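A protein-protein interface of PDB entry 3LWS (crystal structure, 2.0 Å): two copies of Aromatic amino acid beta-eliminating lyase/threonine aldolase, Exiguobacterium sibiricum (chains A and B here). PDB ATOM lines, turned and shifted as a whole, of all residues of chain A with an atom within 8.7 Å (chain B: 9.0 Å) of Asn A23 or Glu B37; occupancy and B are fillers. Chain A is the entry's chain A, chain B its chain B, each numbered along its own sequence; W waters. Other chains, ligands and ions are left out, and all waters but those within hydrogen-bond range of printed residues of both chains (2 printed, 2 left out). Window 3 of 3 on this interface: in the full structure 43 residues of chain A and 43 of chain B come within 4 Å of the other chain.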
ATOM      1  N   HIS A  19     -14.408 -18.787 -11.287  1.00  0.00           N
ATOM      2  CA  HIS A  19     -15.588 -19.463 -11.720  1.00  0.00           C
ATOM      3  C   HIS A  19     -15.390 -20.943 -11.932  1.00  0.00           C
ATOM      4  O   HIS A  19     -16.349 -21.629 -12.259  1.00  0.00           O
ATOM      5  CB  HIS A  19     -16.060 -18.846 -13.032  1.00  0.00           C
ATOM      6  CG  HIS A  19     -16.771 -17.554 -12.854  1.00  0.00           C
ATOM      7  ND1 HIS A  19     -17.813 -17.400 -11.970  1.00  0.00           N
ATOM      8  CD2 HIS A  19     -16.615 -16.359 -13.466  1.00  0.00           C
ATOM      9  CE1 HIS A  19     -18.246 -16.152 -12.021  1.00  0.00           C
ATOM     10  NE2 HIS A  19     -17.530 -15.497 -12.914  1.00  0.00           N
ATOM     11  N   GLY A  20     -14.156 -21.424 -11.767  1.00  0.00           N
ATOM     12  CA  GLY A  20     -13.785 -22.748 -12.235  1.00  0.00           C
ATOM     13  C   GLY A  20     -12.756 -22.676 -13.341  1.00  0.00           C
ATOM     14  O   GLY A  20     -12.302 -21.596 -13.724  1.00  0.00           O
ATOM     15  N   LYS A  21     -12.360 -23.834 -13.836  1.00  0.00           N
ATOM     16  CA  LYS A  21     -11.310 -23.904 -14.835  1.00  0.00           C
ATOM     17  C   LYS A  21     -11.747 -23.265 -16.132  1.00  0.00           C
ATOM     18  O   LYS A  21     -12.925 -23.370 -16.560  1.00  0.00           O
ATOM     19  CB  LYS A  21     -10.885 -25.354 -15.102  1.00  0.00           C
ATOM     20  CG  LYS A  21      -9.823 -25.891 -14.141  1.00  0.00           C
ATOM     21  CD  LYS A  21     -10.375 -26.698 -12.985  1.00  0.00           C
ATOM     22  CE  LYS A  21      -9.246 -27.380 -12.210  1.00  0.00           C
ATOM     23  NZ  LYS A  21      -8.206 -26.441 -11.733  1.00  0.00           N
ATOM     24  N   ARG A  22     -10.786 -22.617 -16.757  1.00  0.00           N
ATOM     25  CA  ARG A  22     -10.975 -21.935 -18.028  1.00  0.00           C
ATOM     26  C   ARG A  22     -10.729 -22.962 -19.123  1.00  0.00           C
ATOM     27  O   ARG A  22      -9.598 -23.142 -19.594  1.00  0.00           O
ATOM     28  CB  ARG A  22      -9.980 -20.755 -18.132  1.00  0.00           C
ATOM     29  CG  ARG A  22     -10.072 -19.949 -19.415  1.00  0.00           C
ATOM     30  CD  ARG A  22      -9.068 -18.798 -19.491  1.00  0.00           C
ATOM     31  NE  ARG A  22      -9.109 -17.990 -18.283  1.00  0.00           N
ATOM     32  CZ  ARG A  22     -10.052 -17.107 -17.984  1.00  0.00           C
ATOM     33  NH1 ARG A  22     -11.074 -16.871 -18.808  1.00  0.00           N
ATOM     34  NH2 ARG A  22      -9.965 -16.448 -16.834  1.00  0.00           N
ATOM     35  N   ASN A  23     -11.783 -23.661 -19.518  1.00  0.00           N
ATOM     36  CA  ASN A  23     -11.636 -24.714 -20.540  1.00  0.00           C
ATOM     37  C   ASN A  23     -12.641 -24.667 -21.688  1.00  0.00           C
ATOM     38  O   ASN A  23     -13.508 -23.799 -21.728  1.00  0.00           O
ATOM     39  CB  ASN A  23     -11.612 -26.094 -19.858  1.00  0.00           C
ATOM     40  CG  ASN A  23     -12.797 -26.337 -18.978  1.00  0.00           C
ATOM     41  OD1 ASN A  23     -13.918 -25.838 -19.216  1.00  0.00           O
ATOM     42  ND2 ASN A  23     -12.579 -27.149 -17.968  1.00  0.00           N
ATOM     43  N   VAL A  24     -12.490 -25.609 -22.627  1.00  0.00           N
ATOM     44  CA  VAL A  24     -13.307 -25.729 -23.819  1.00  0.00           C
ATOM     45  C   VAL A  24     -14.773 -25.921 -23.466  1.00  0.00           C
ATOM     46  O   VAL A  24     -15.635 -25.448 -24.198  1.00  0.00           O
ATOM     47  CB  VAL A  24     -12.786 -26.924 -24.729  1.00  0.00           C
ATOM     48  CG1 VAL A  24     -13.831 -27.379 -25.713  1.00  0.00           C
ATOM     49  CG2 VAL A  24     -11.496 -26.513 -25.480  1.00  0.00           C
ATOM     50  N   GLY A  25     -15.043 -26.600 -22.339  1.00  0.00           N
ATOM     51  CA  GLY A  25     -16.404 -26.751 -21.824  1.00  0.00           C
ATOM     52  C   GLY A  25     -17.184 -25.450 -21.653  1.00  0.00           C
ATOM     53  O   GLY A  25     -18.408 -25.443 -21.809  1.00  0.00           O
ATOM     54  N   VAL A  26     -16.491 -24.361 -21.300  1.00  0.00           N
ATOM     55  CA  VAL A  26     -17.139 -23.026 -21.197  1.00  0.00           C
ATOM     56  C   VAL A  26     -17.845 -22.662 -22.521  1.00  0.00           C
ATOM     57  O   VAL A  26     -18.978 -22.222 -22.521  1.00  0.00           O
ATOM     58  CB  VAL A  26     -16.124 -21.934 -20.768  1.00  0.00           C
ATOM     59  CG1 VAL A  26     -16.732 -20.514 -20.864  1.00  0.00           C
ATOM     60  CG2 VAL A  26     -15.608 -22.195 -19.324  1.00  0.00           C
ATOM     61  N   LEU A  27     -17.178 -22.891 -23.653  1.00  0.00           N
ATOM     62  CA  LEU A  27     -17.796 -22.628 -24.979  1.00  0.00           C
ATOM     63  C   LEU A  27     -18.837 -23.691 -25.261  1.00  0.00           C
ATOM     64  O   LEU A  27     -19.968 -23.348 -25.537  1.00  0.00           O
ATOM     65  CB  LEU A  27     -16.767 -22.546 -26.124  1.00  0.00           C
ATOM     66  CG  LEU A  27     -17.204 -22.112 -27.550  1.00  0.00           C
ATOM     67  CD1 LEU A  27     -17.684 -20.667 -27.655  1.00  0.00           C
ATOM     68  CD2 LEU A  27     -16.046 -22.320 -28.525  1.00  0.00           C
ATOM     69  N   LYS A  28     -18.496 -24.978 -25.088  1.00  0.00           N
ATOM     70  CA  LYS A  28     -19.474 -26.030 -25.375  1.00  0.00           C
ATOM     71  C   LYS A  28     -20.761 -25.855 -24.575  1.00  0.00           C
ATOM     72  O   LYS A  28     -21.831 -25.977 -25.125  1.00  0.00           O
ATOM     73  CB  LYS A  28     -18.891 -27.438 -25.257  1.00  0.00           C
ATOM     74  CG  LYS A  28     -17.820 -27.719 -26.327  1.00  0.00           C
ATOM     75  CD  LYS A  28     -17.289 -29.137 -26.292  1.00  0.00           C
ATOM     76  CE  LYS A  28     -18.323 -30.155 -26.684  1.00  0.00           C
ATOM     77  NZ  LYS A  28     -17.750 -31.428 -27.127  1.00  0.00           N
ATOM     78  N   THR A  29     -20.660 -25.484 -23.318  1.00  0.00           N
ATOM     79  CA  THR A  29     -21.850 -25.252 -22.536  1.00  0.00           C
ATOM     80  C   THR A  29     -22.703 -24.107 -23.111  1.00  0.00           C
ATOM     81  O   THR A  29     -23.909 -24.250 -23.210  1.00  0.00           O
ATOM     82  CB  THR A  29     -21.557 -24.961 -21.091  1.00  0.00           C
ATOM     83  OG1 THR A  29     -20.891 -26.078 -20.513  1.00  0.00           O
ATOM     84  CG2 THR A  29     -22.868 -24.700 -20.328  1.00  0.00           C
ATOM     85  N   GLY A 209     -17.634 -14.080 -16.576  1.00  0.00           N
ATOM     86  CA  GLY A 209     -17.044 -15.396 -16.812  1.00  0.00           C
ATOM     87  C   GLY A 209     -17.305 -16.049 -18.161  1.00  0.00           C
ATOM     88  O   GLY A 209     -17.315 -17.284 -18.274  1.00  0.00           O
ATOM     89  N   GLY A 210     -17.491 -15.232 -19.187  1.00  0.00           N
ATOM     90  CA  GLY A 210     -17.529 -15.709 -20.565  1.00  0.00           C
ATOM     91  C   GLY A 210     -16.098 -15.981 -21.022  1.00  0.00           C
ATOM     92  O   GLY A 210     -15.172 -16.059 -20.216  1.00  0.00           O
ATOM     93  N   ILE A 211     -15.912 -16.090 -22.324  1.00  0.00           N
ATOM     94  CA  ILE A 211     -14.636 -16.509 -22.914  1.00  0.00           C
ATOM     95  C   ILE A 211     -13.766 -15.332 -23.322  1.00  0.00           C
ATOM     96  O   ILE A 211     -12.551 -15.290 -23.043  1.00  0.00           O
ATOM     97  CB  ILE A 211     -14.907 -17.411 -24.111  1.00  0.00           C
ATOM     98  CG1 ILE A 211     -15.519 -18.722 -23.580  1.00  0.00           C
ATOM     99  CG2 ILE A 211     -13.612 -17.695 -24.915  1.00  0.00           C
ATOM    100  CD1 ILE A 211     -16.086 -19.645 -24.669  1.00  0.00           C
ATOM    101  N   TYR A 250     -23.395 -16.249 -20.798  1.00  0.00           N
ATOM    102  CA  TYR A 250     -22.852 -16.055 -19.424  1.00  0.00           C
ATOM    103  C   TYR A 250     -23.413 -14.799 -18.797  1.00  0.00           C
ATOM    104  O   TYR A 250     -23.566 -14.725 -17.580  1.00  0.00           O
ATOM    105  CB  TYR A 250     -21.320 -16.169 -19.390  1.00  0.00           C
ATOM    106  CG  TYR A 250     -20.944 -17.608 -19.648  1.00  0.00           C
ATOM    107  CD1 TYR A 250     -21.192 -18.590 -18.694  1.00  0.00           C
ATOM    108  CD2 TYR A 250     -20.403 -18.009 -20.857  1.00  0.00           C
ATOM    109  CE1 TYR A 250     -20.908 -19.897 -18.936  1.00  0.00           C
ATOM    110  CE2 TYR A 250     -20.111 -19.322 -21.100  1.00  0.00           C
ATOM    111  CZ  TYR A 250     -20.379 -20.259 -20.154  1.00  0.00           C
ATOM    112  OH  TYR A 250     -20.068 -21.571 -20.387  1.00  0.00           O
ATOM    113  N   PHE B  31     -16.036 -28.820 -32.623  1.00  0.00           N
ATOM    114  CA  PHE B  31     -15.843 -29.061 -31.206  1.00  0.00           C
ATOM    115  C   PHE B  31     -16.437 -30.430 -30.729  1.00  0.00           C
ATOM    116  O   PHE B  31     -16.178 -30.823 -29.588  1.00  0.00           O
ATOM    117  CB  PHE B  31     -16.386 -27.882 -30.358  1.00  0.00           C
ATOM    118  CG  PHE B  31     -15.394 -26.732 -30.223  1.00  0.00           C
ATOM    119  CD1 PHE B  31     -15.248 -25.782 -31.225  1.00  0.00           C
ATOM    120  CD2 PHE B  31     -14.556 -26.668 -29.136  1.00  0.00           C
ATOM    121  CE1 PHE B  31     -14.309 -24.769 -31.102  1.00  0.00           C
ATOM    122  CE2 PHE B  31     -13.587 -25.665 -29.006  1.00  0.00           C
ATOM    123  CZ  PHE B  31     -13.463 -24.712 -29.974  1.00  0.00           C
ATOM    124  N   ALA B  33     -15.841 -33.483 -30.887  1.00  0.00           N
ATOM    125  CA  ALA B  33     -14.861 -34.433 -30.330  1.00  0.00           C
ATOM    126  C   ALA B  33     -13.782 -33.830 -29.412  1.00  0.00           C
ATOM    127  O   ALA B  33     -12.861 -34.550 -29.024  1.00  0.00           O
ATOM    128  CB  ALA B  33     -14.179 -35.201 -31.472  1.00  0.00           C
ATOM    129  N   VAL B  34     -13.871 -32.547 -29.043  1.00  0.00           N
ATOM    130  CA  VAL B  34     -12.899 -31.993 -28.090  1.00  0.00           C
ATOM    131  C   VAL B  34     -13.486 -32.100 -26.703  1.00  0.00           C
ATOM    132  O   VAL B  34     -14.607 -31.657 -26.468  1.00  0.00           O
ATOM    133  CB  VAL B  34     -12.476 -30.507 -28.409  1.00  0.00           C
ATOM    134  CG1 VAL B  34     -11.501 -29.989 -27.359  1.00  0.00           C
ATOM    135  CG2 VAL B  34     -11.835 -30.410 -29.761  1.00  0.00           C
ATOM    136  N   ALA B  35     -12.744 -32.726 -25.797  1.00  0.00           N
ATOM    137  CA  ALA B  35     -13.162 -32.854 -24.390  1.00  0.00           C
ATOM    138  C   ALA B  35     -13.399 -31.480 -23.781  1.00  0.00           C
ATOM    139  O   ALA B  35     -12.603 -30.548 -24.034  1.00  0.00           O
ATOM    140  CB  ALA B  35     -12.117 -33.620 -23.573  1.00  0.00           C
ATOM    141  N   ASP B  36     -14.483 -31.363 -22.998  1.00  0.00           N
ATOM    142  CA  ASP B  36     -14.779 -30.170 -22.181  1.00  0.00           C
ATOM    143  C   ASP B  36     -13.589 -29.709 -21.319  1.00  0.00           C
ATOM    144  O   ASP B  36     -13.428 -28.518 -21.069  1.00  0.00           O
ATOM    145  CB  ASP B  36     -15.985 -30.407 -21.256  1.00  0.00           C
ATOM    146  CG  ASP B  36     -17.327 -30.465 -21.986  1.00  0.00           C
ATOM    147  OD1 ASP B  36     -17.421 -30.116 -23.179  1.00  0.00           O
ATOM    148  OD2 ASP B  36     -18.321 -30.880 -21.342  1.00  0.00           O
ATOM    149  N   GLU B  37     -12.758 -30.645 -20.851  1.00  0.00           N
ATOM    150  CA  GLU B  37     -11.699 -30.333 -19.884  1.00  0.00           C
ATOM    151  C   GLU B  37     -10.427 -29.756 -20.510  1.00  0.00           C
ATOM    152  O   GLU B  37      -9.518 -29.373 -19.789  1.00  0.00           O
ATOM    153  CB  GLU B  37     -11.290 -31.578 -19.087  1.00  0.00           C
ATOM    154  CG  GLU B  37     -12.463 -32.370 -18.524  1.00  0.00           C
ATOM    155  CD  GLU B  37     -12.963 -33.457 -19.493  1.00  0.00           C
ATOM    156  OE1 GLU B  37     -12.449 -34.611 -19.450  1.00  0.00           O
ATOM    157  OE2 GLU B  37     -13.876 -33.144 -20.294  1.00  0.00           O
ATOM    158  N   MET B  38     -10.354 -29.694 -21.829  1.00  0.00           N
ATOM    159  CA  MET B  38      -9.169 -29.186 -22.504  1.00  0.00           C
ATOM    160  C   MET B  38      -8.945 -27.761 -22.049  1.00  0.00           C
ATOM    161  O   MET B  38      -9.875 -26.957 -22.071  1.00  0.00           O
ATOM    162  CB  MET B  38      -9.323 -29.230 -24.030  1.00  0.00           C
ATOM    163  CG  MET B  38      -8.155 -28.609 -24.817  1.00  0.00           C
ATOM    164  SD  MET B  38      -8.062 -29.000 -26.765  1.00  0.00           S
ATOM    165  CE  MET B  38      -6.112 -29.183 -26.785  1.00  0.00           C
ATOM    166  N   ALA B  39      -7.721 -27.466 -21.634  1.00  0.00           N
ATOM    167  CA  ALA B  39      -7.311 -26.145 -21.221  1.00  0.00           C
ATOM    168  C   ALA B  39      -7.403 -25.143 -22.383  1.00  0.00           C
ATOM    169  O   ALA B  39      -6.989 -25.453 -23.492  1.00  0.00           O
ATOM    170  CB  ALA B  39      -5.851 -26.200 -20.709  1.00  0.00           C
ATOM    171  N   SER B  40      -7.899 -23.943 -22.097  1.00  0.00           N
ATOM    172  CA  SER B  40      -7.843 -22.815 -23.026  1.00  0.00           C
ATOM    173  C   SER B  40      -6.394 -22.401 -23.243  1.00  0.00           C
ATOM    174  O   SER B  40      -5.524 -22.619 -22.403  1.00  0.00           O
ATOM    175  CB  SER B  40      -8.637 -21.628 -22.463  1.00  0.00           C
ATOM    176  OG  SER B  40      -8.481 -20.421 -23.227  1.00  0.00           O
ATOM    177  N   ASP B  41      -6.125 -21.775 -24.375  1.00  0.00           N
ATOM    178  CA  ASP B  41      -4.912 -20.932 -24.488  1.00  0.00           C
ATOM    179  C   ASP B  41      -5.027 -19.813 -23.471  1.00  0.00           C
ATOM    180  O   ASP B  41      -6.093 -19.653 -22.874  1.00  0.00           O
ATOM    181  CB  ASP B  41      -4.745 -20.374 -25.919  1.00  0.00           C
ATOM    182  CG  ASP B  41      -5.972 -19.670 -26.432  1.00  0.00           C
ATOM    183  OD1 ASP B  41      -7.127 -20.087 -26.190  1.00  0.00           O
ATOM    184  OD2 ASP B  41      -5.794 -18.690 -27.134  1.00  0.00           O
ATOM    185  N   ALA B  47      -1.679 -23.885 -23.758  1.00  0.00           N
ATOM    186  CA  ALA B  47      -2.438 -24.960 -24.409  1.00  0.00           C
ATOM    187  C   ALA B  47      -3.109 -24.499 -25.711  1.00  0.00           C
ATOM    188  O   ALA B  47      -3.610 -23.362 -25.806  1.00  0.00           O
ATOM    189  CB  ALA B  47      -3.487 -25.521 -23.463  1.00  0.00           C
ATOM    190  N   ILE B  48      -3.084 -25.378 -26.714  1.00  0.00           N
ATOM    191  CA  ILE B  48      -3.844 -25.237 -27.945  1.00  0.00           C
ATOM    192  C   ILE B  48      -3.124 -24.376 -28.975  1.00  0.00           C
ATOM    193  O   ILE B  48      -2.876 -24.816 -30.104  1.00  0.00           O
ATOM    194  CB  ILE B  48      -5.301 -24.724 -27.721  1.00  0.00           C
ATOM    195  CG1 ILE B  48      -6.086 -25.757 -26.888  1.00  0.00           C
ATOM    196  CG2 ILE B  48      -5.951 -24.461 -29.090  1.00  0.00           C
ATOM    197  CD1 ILE B  48      -7.529 -25.359 -26.512  1.00  0.00           C
ATOM    198  N   SER B 239      -8.416 -15.874 -24.852  1.00  0.00           N
ATOM    199  CA  SER B 239      -8.716 -17.194 -25.398  1.00  0.00           C
ATOM    200  C   SER B 239      -9.070 -17.101 -26.857  1.00  0.00           C
ATOM    201  O   SER B 239     -10.167 -16.651 -27.188  1.00  0.00           O
ATOM    202  CB  SER B 239      -9.873 -17.847 -24.619  1.00  0.00           C
ATOM    203  OG  SER B 239      -9.502 -18.098 -23.270  1.00  0.00           O
ATOM    204  N   TYR B 241      -8.820 -20.064 -28.690  1.00  0.00           N
ATOM    205  CA  TYR B 241      -9.170 -21.473 -29.046  1.00  0.00           C
ATOM    206  C   TYR B 241     -10.457 -21.686 -29.835  1.00  0.00           C
ATOM    207  O   TYR B 241     -10.494 -22.601 -30.630  1.00  0.00           O
ATOM    208  CB  TYR B 241      -9.229 -22.425 -27.826  1.00  0.00           C
ATOM    209  CG  TYR B 241     -10.417 -22.224 -26.915  1.00  0.00           C
ATOM    210  CD1 TYR B 241     -11.637 -22.867 -27.133  1.00  0.00           C
ATOM    211  CD2 TYR B 241     -10.291 -21.447 -25.776  1.00  0.00           C
ATOM    212  CE1 TYR B 241     -12.712 -22.665 -26.265  1.00  0.00           C
ATOM    213  CE2 TYR B 241     -11.322 -21.242 -24.924  1.00  0.00           C
ATOM    214  CZ  TYR B 241     -12.542 -21.860 -25.150  1.00  0.00           C
ATOM    215  OH  TYR B 241     -13.543 -21.587 -24.248  1.00  0.00           O
ATOM    216  N   PRO B 242     -11.506 -20.850 -29.643  1.00  0.00           N
ATOM    217  CA  PRO B 242     -12.635 -21.136 -30.527  1.00  0.00           C
ATOM    218  C   PRO B 242     -12.289 -21.100 -32.023  1.00  0.00           C
ATOM    219  O   PRO B 242     -12.881 -21.849 -32.805  1.00  0.00           O
ATOM    220  CB  PRO B 242     -13.647 -20.078 -30.160  1.00  0.00           C
ATOM    221  CG  PRO B 242     -13.272 -19.653 -28.807  1.00  0.00           C
ATOM    222  CD  PRO B 242     -11.816 -19.736 -28.733  1.00  0.00           C
HETATM  223  O   HOH W   1      -6.493 -22.009 -19.362  1.00  0.00           O
HETATM  224  O   HOH W   2     -12.726 -21.229 -21.880  1.00  0.00           O
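Of the printed residues of chain B, Asn A23 touches Asp B36 (3.1 Å), Glu B37 (3.8 Å), Met B38 (2.9 Å) and Tyr B241 (3.4 Å).
Glu B37 touches one residue of chain A.
Printed residues of chain B within 4 Å of Leu A27: Phe B31, Tyr B241 and Pro B242.
Printed residues of chain A within 4 Å of Met B38: Asn A23 and Val A24.
Printed residues of chain A within 4 Å of Pro B242: Leu A27 (3.7 Å).
Val A26 touches none of the printed residues of chain B.
Asp B41 touches none of the printed residues of chain A.
The nearest printed residue of chain A that does not touch Phe B31 is Gly A25 (6.8 Å).
No position is printed for both chains.
Arg A22 touches Ser B239 (CD to OG, 3.9 Å).
Asn A23 touches Glu B37 (ND2 to CA, 3.8 Å).
CB of Asn A23 touches O of Met B38 (2.9 Å).
Val B34 touches Val A24 (CG1 to CG1, 3.9 Å).
CB of Val A24 touches O of Ala B35, at 3.7 Å.
CA of Val A24 touches CE1 of Tyr B241, 3.97 Å away.
Leu A27 touches Phe B31.
Pro B242 touches Leu A27 (CB to CD2, 3.7 Å).
Lys A28 touches Asp B36.
CD1 of Ile A211 touches OH of Tyr B241, 3.2 Å away.
Of the 15 printed residues of chain B, 10 touch a printed residue of chain A.
Hydrophobic or aromatic side chains of chain B that line the printed part of chain A: Phe B31, Val B34, Met B38, Tyr B241 and Pro B242.
Of the 15 printed residues of chain A, 7 touch a printed residue of chain B.
Hydrophobic or aromatic side chains of chain A that line the printed part of chain B: Val A24, Leu A27 and Ile A211.
Among the printed residues, 21 pairs touch across the chains.
Water W2 bridges the side-chain hydroxyl of Tyr B241 (2.5 Å) and the backbone carbonyl oxygen of Asn A23 (2.7 Å).
Water W1 lies within hydrogen-bond range of the backbone carbonyl oxygen of Ser B40 and the backbone carbonyl oxygen of Arg A22.
The backbone carbonyl oxygen (O) of Arg A22 lies within hydrogen-bond range of the backbone NH (N) of Ser B40 (3.1 Å).
OD1 of Asn A23 lies close to O of Asp B36.
O of Asn A23 sits at hydrogen-bond distance from OH of Tyr B241, 3.4 Å away.
The backbone carbonyl oxygen (O) of Asp B36 sits at hydrogen-bond distance from the backbone NH (N) of Val A24 (3.4 Å).
The backbone NH (N) of Val A24 is in hydrogen-bond range of the backbone carbonyl oxygen (O) of Met B38 (3.0 Å).
The backbone carbonyl oxygen (O) of Asp B36 is in hydrogen-bond range of the backbone NH (N) of Gly A25.
NZ of Lys A28 is in hydrogen-bond range of O of Phe B31.
The side-chain amino group (NZ) of Lys A28 sits at hydrogen-bond distance from the backbone carbonyl oxygen (O) of Val B34 (3.2 Å).
The backbone NH (N) of Gly A25 lies close to the side-chain amide oxygen (OD1) of Asn A23 (3.4 Å).
The side-chain hydroxyl of Thr A29 sits at hydrogen-bond distance from the backbone carbonyl oxygen of Gly A25, 2.9 Å away.
The side-chain carboxylate (OD1) of Asp B41 is in hydrogen-bond range of the side-chain hydroxyl (OG) of Ser B40, at 3.3 Å.
OG of Ser B40 is in hydrogen-bond range of OG of Ser B239, at 2.5 Å.
OD1 of Asp B41 is in hydrogen-bond range of N of Tyr B241 (3.0 Å).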
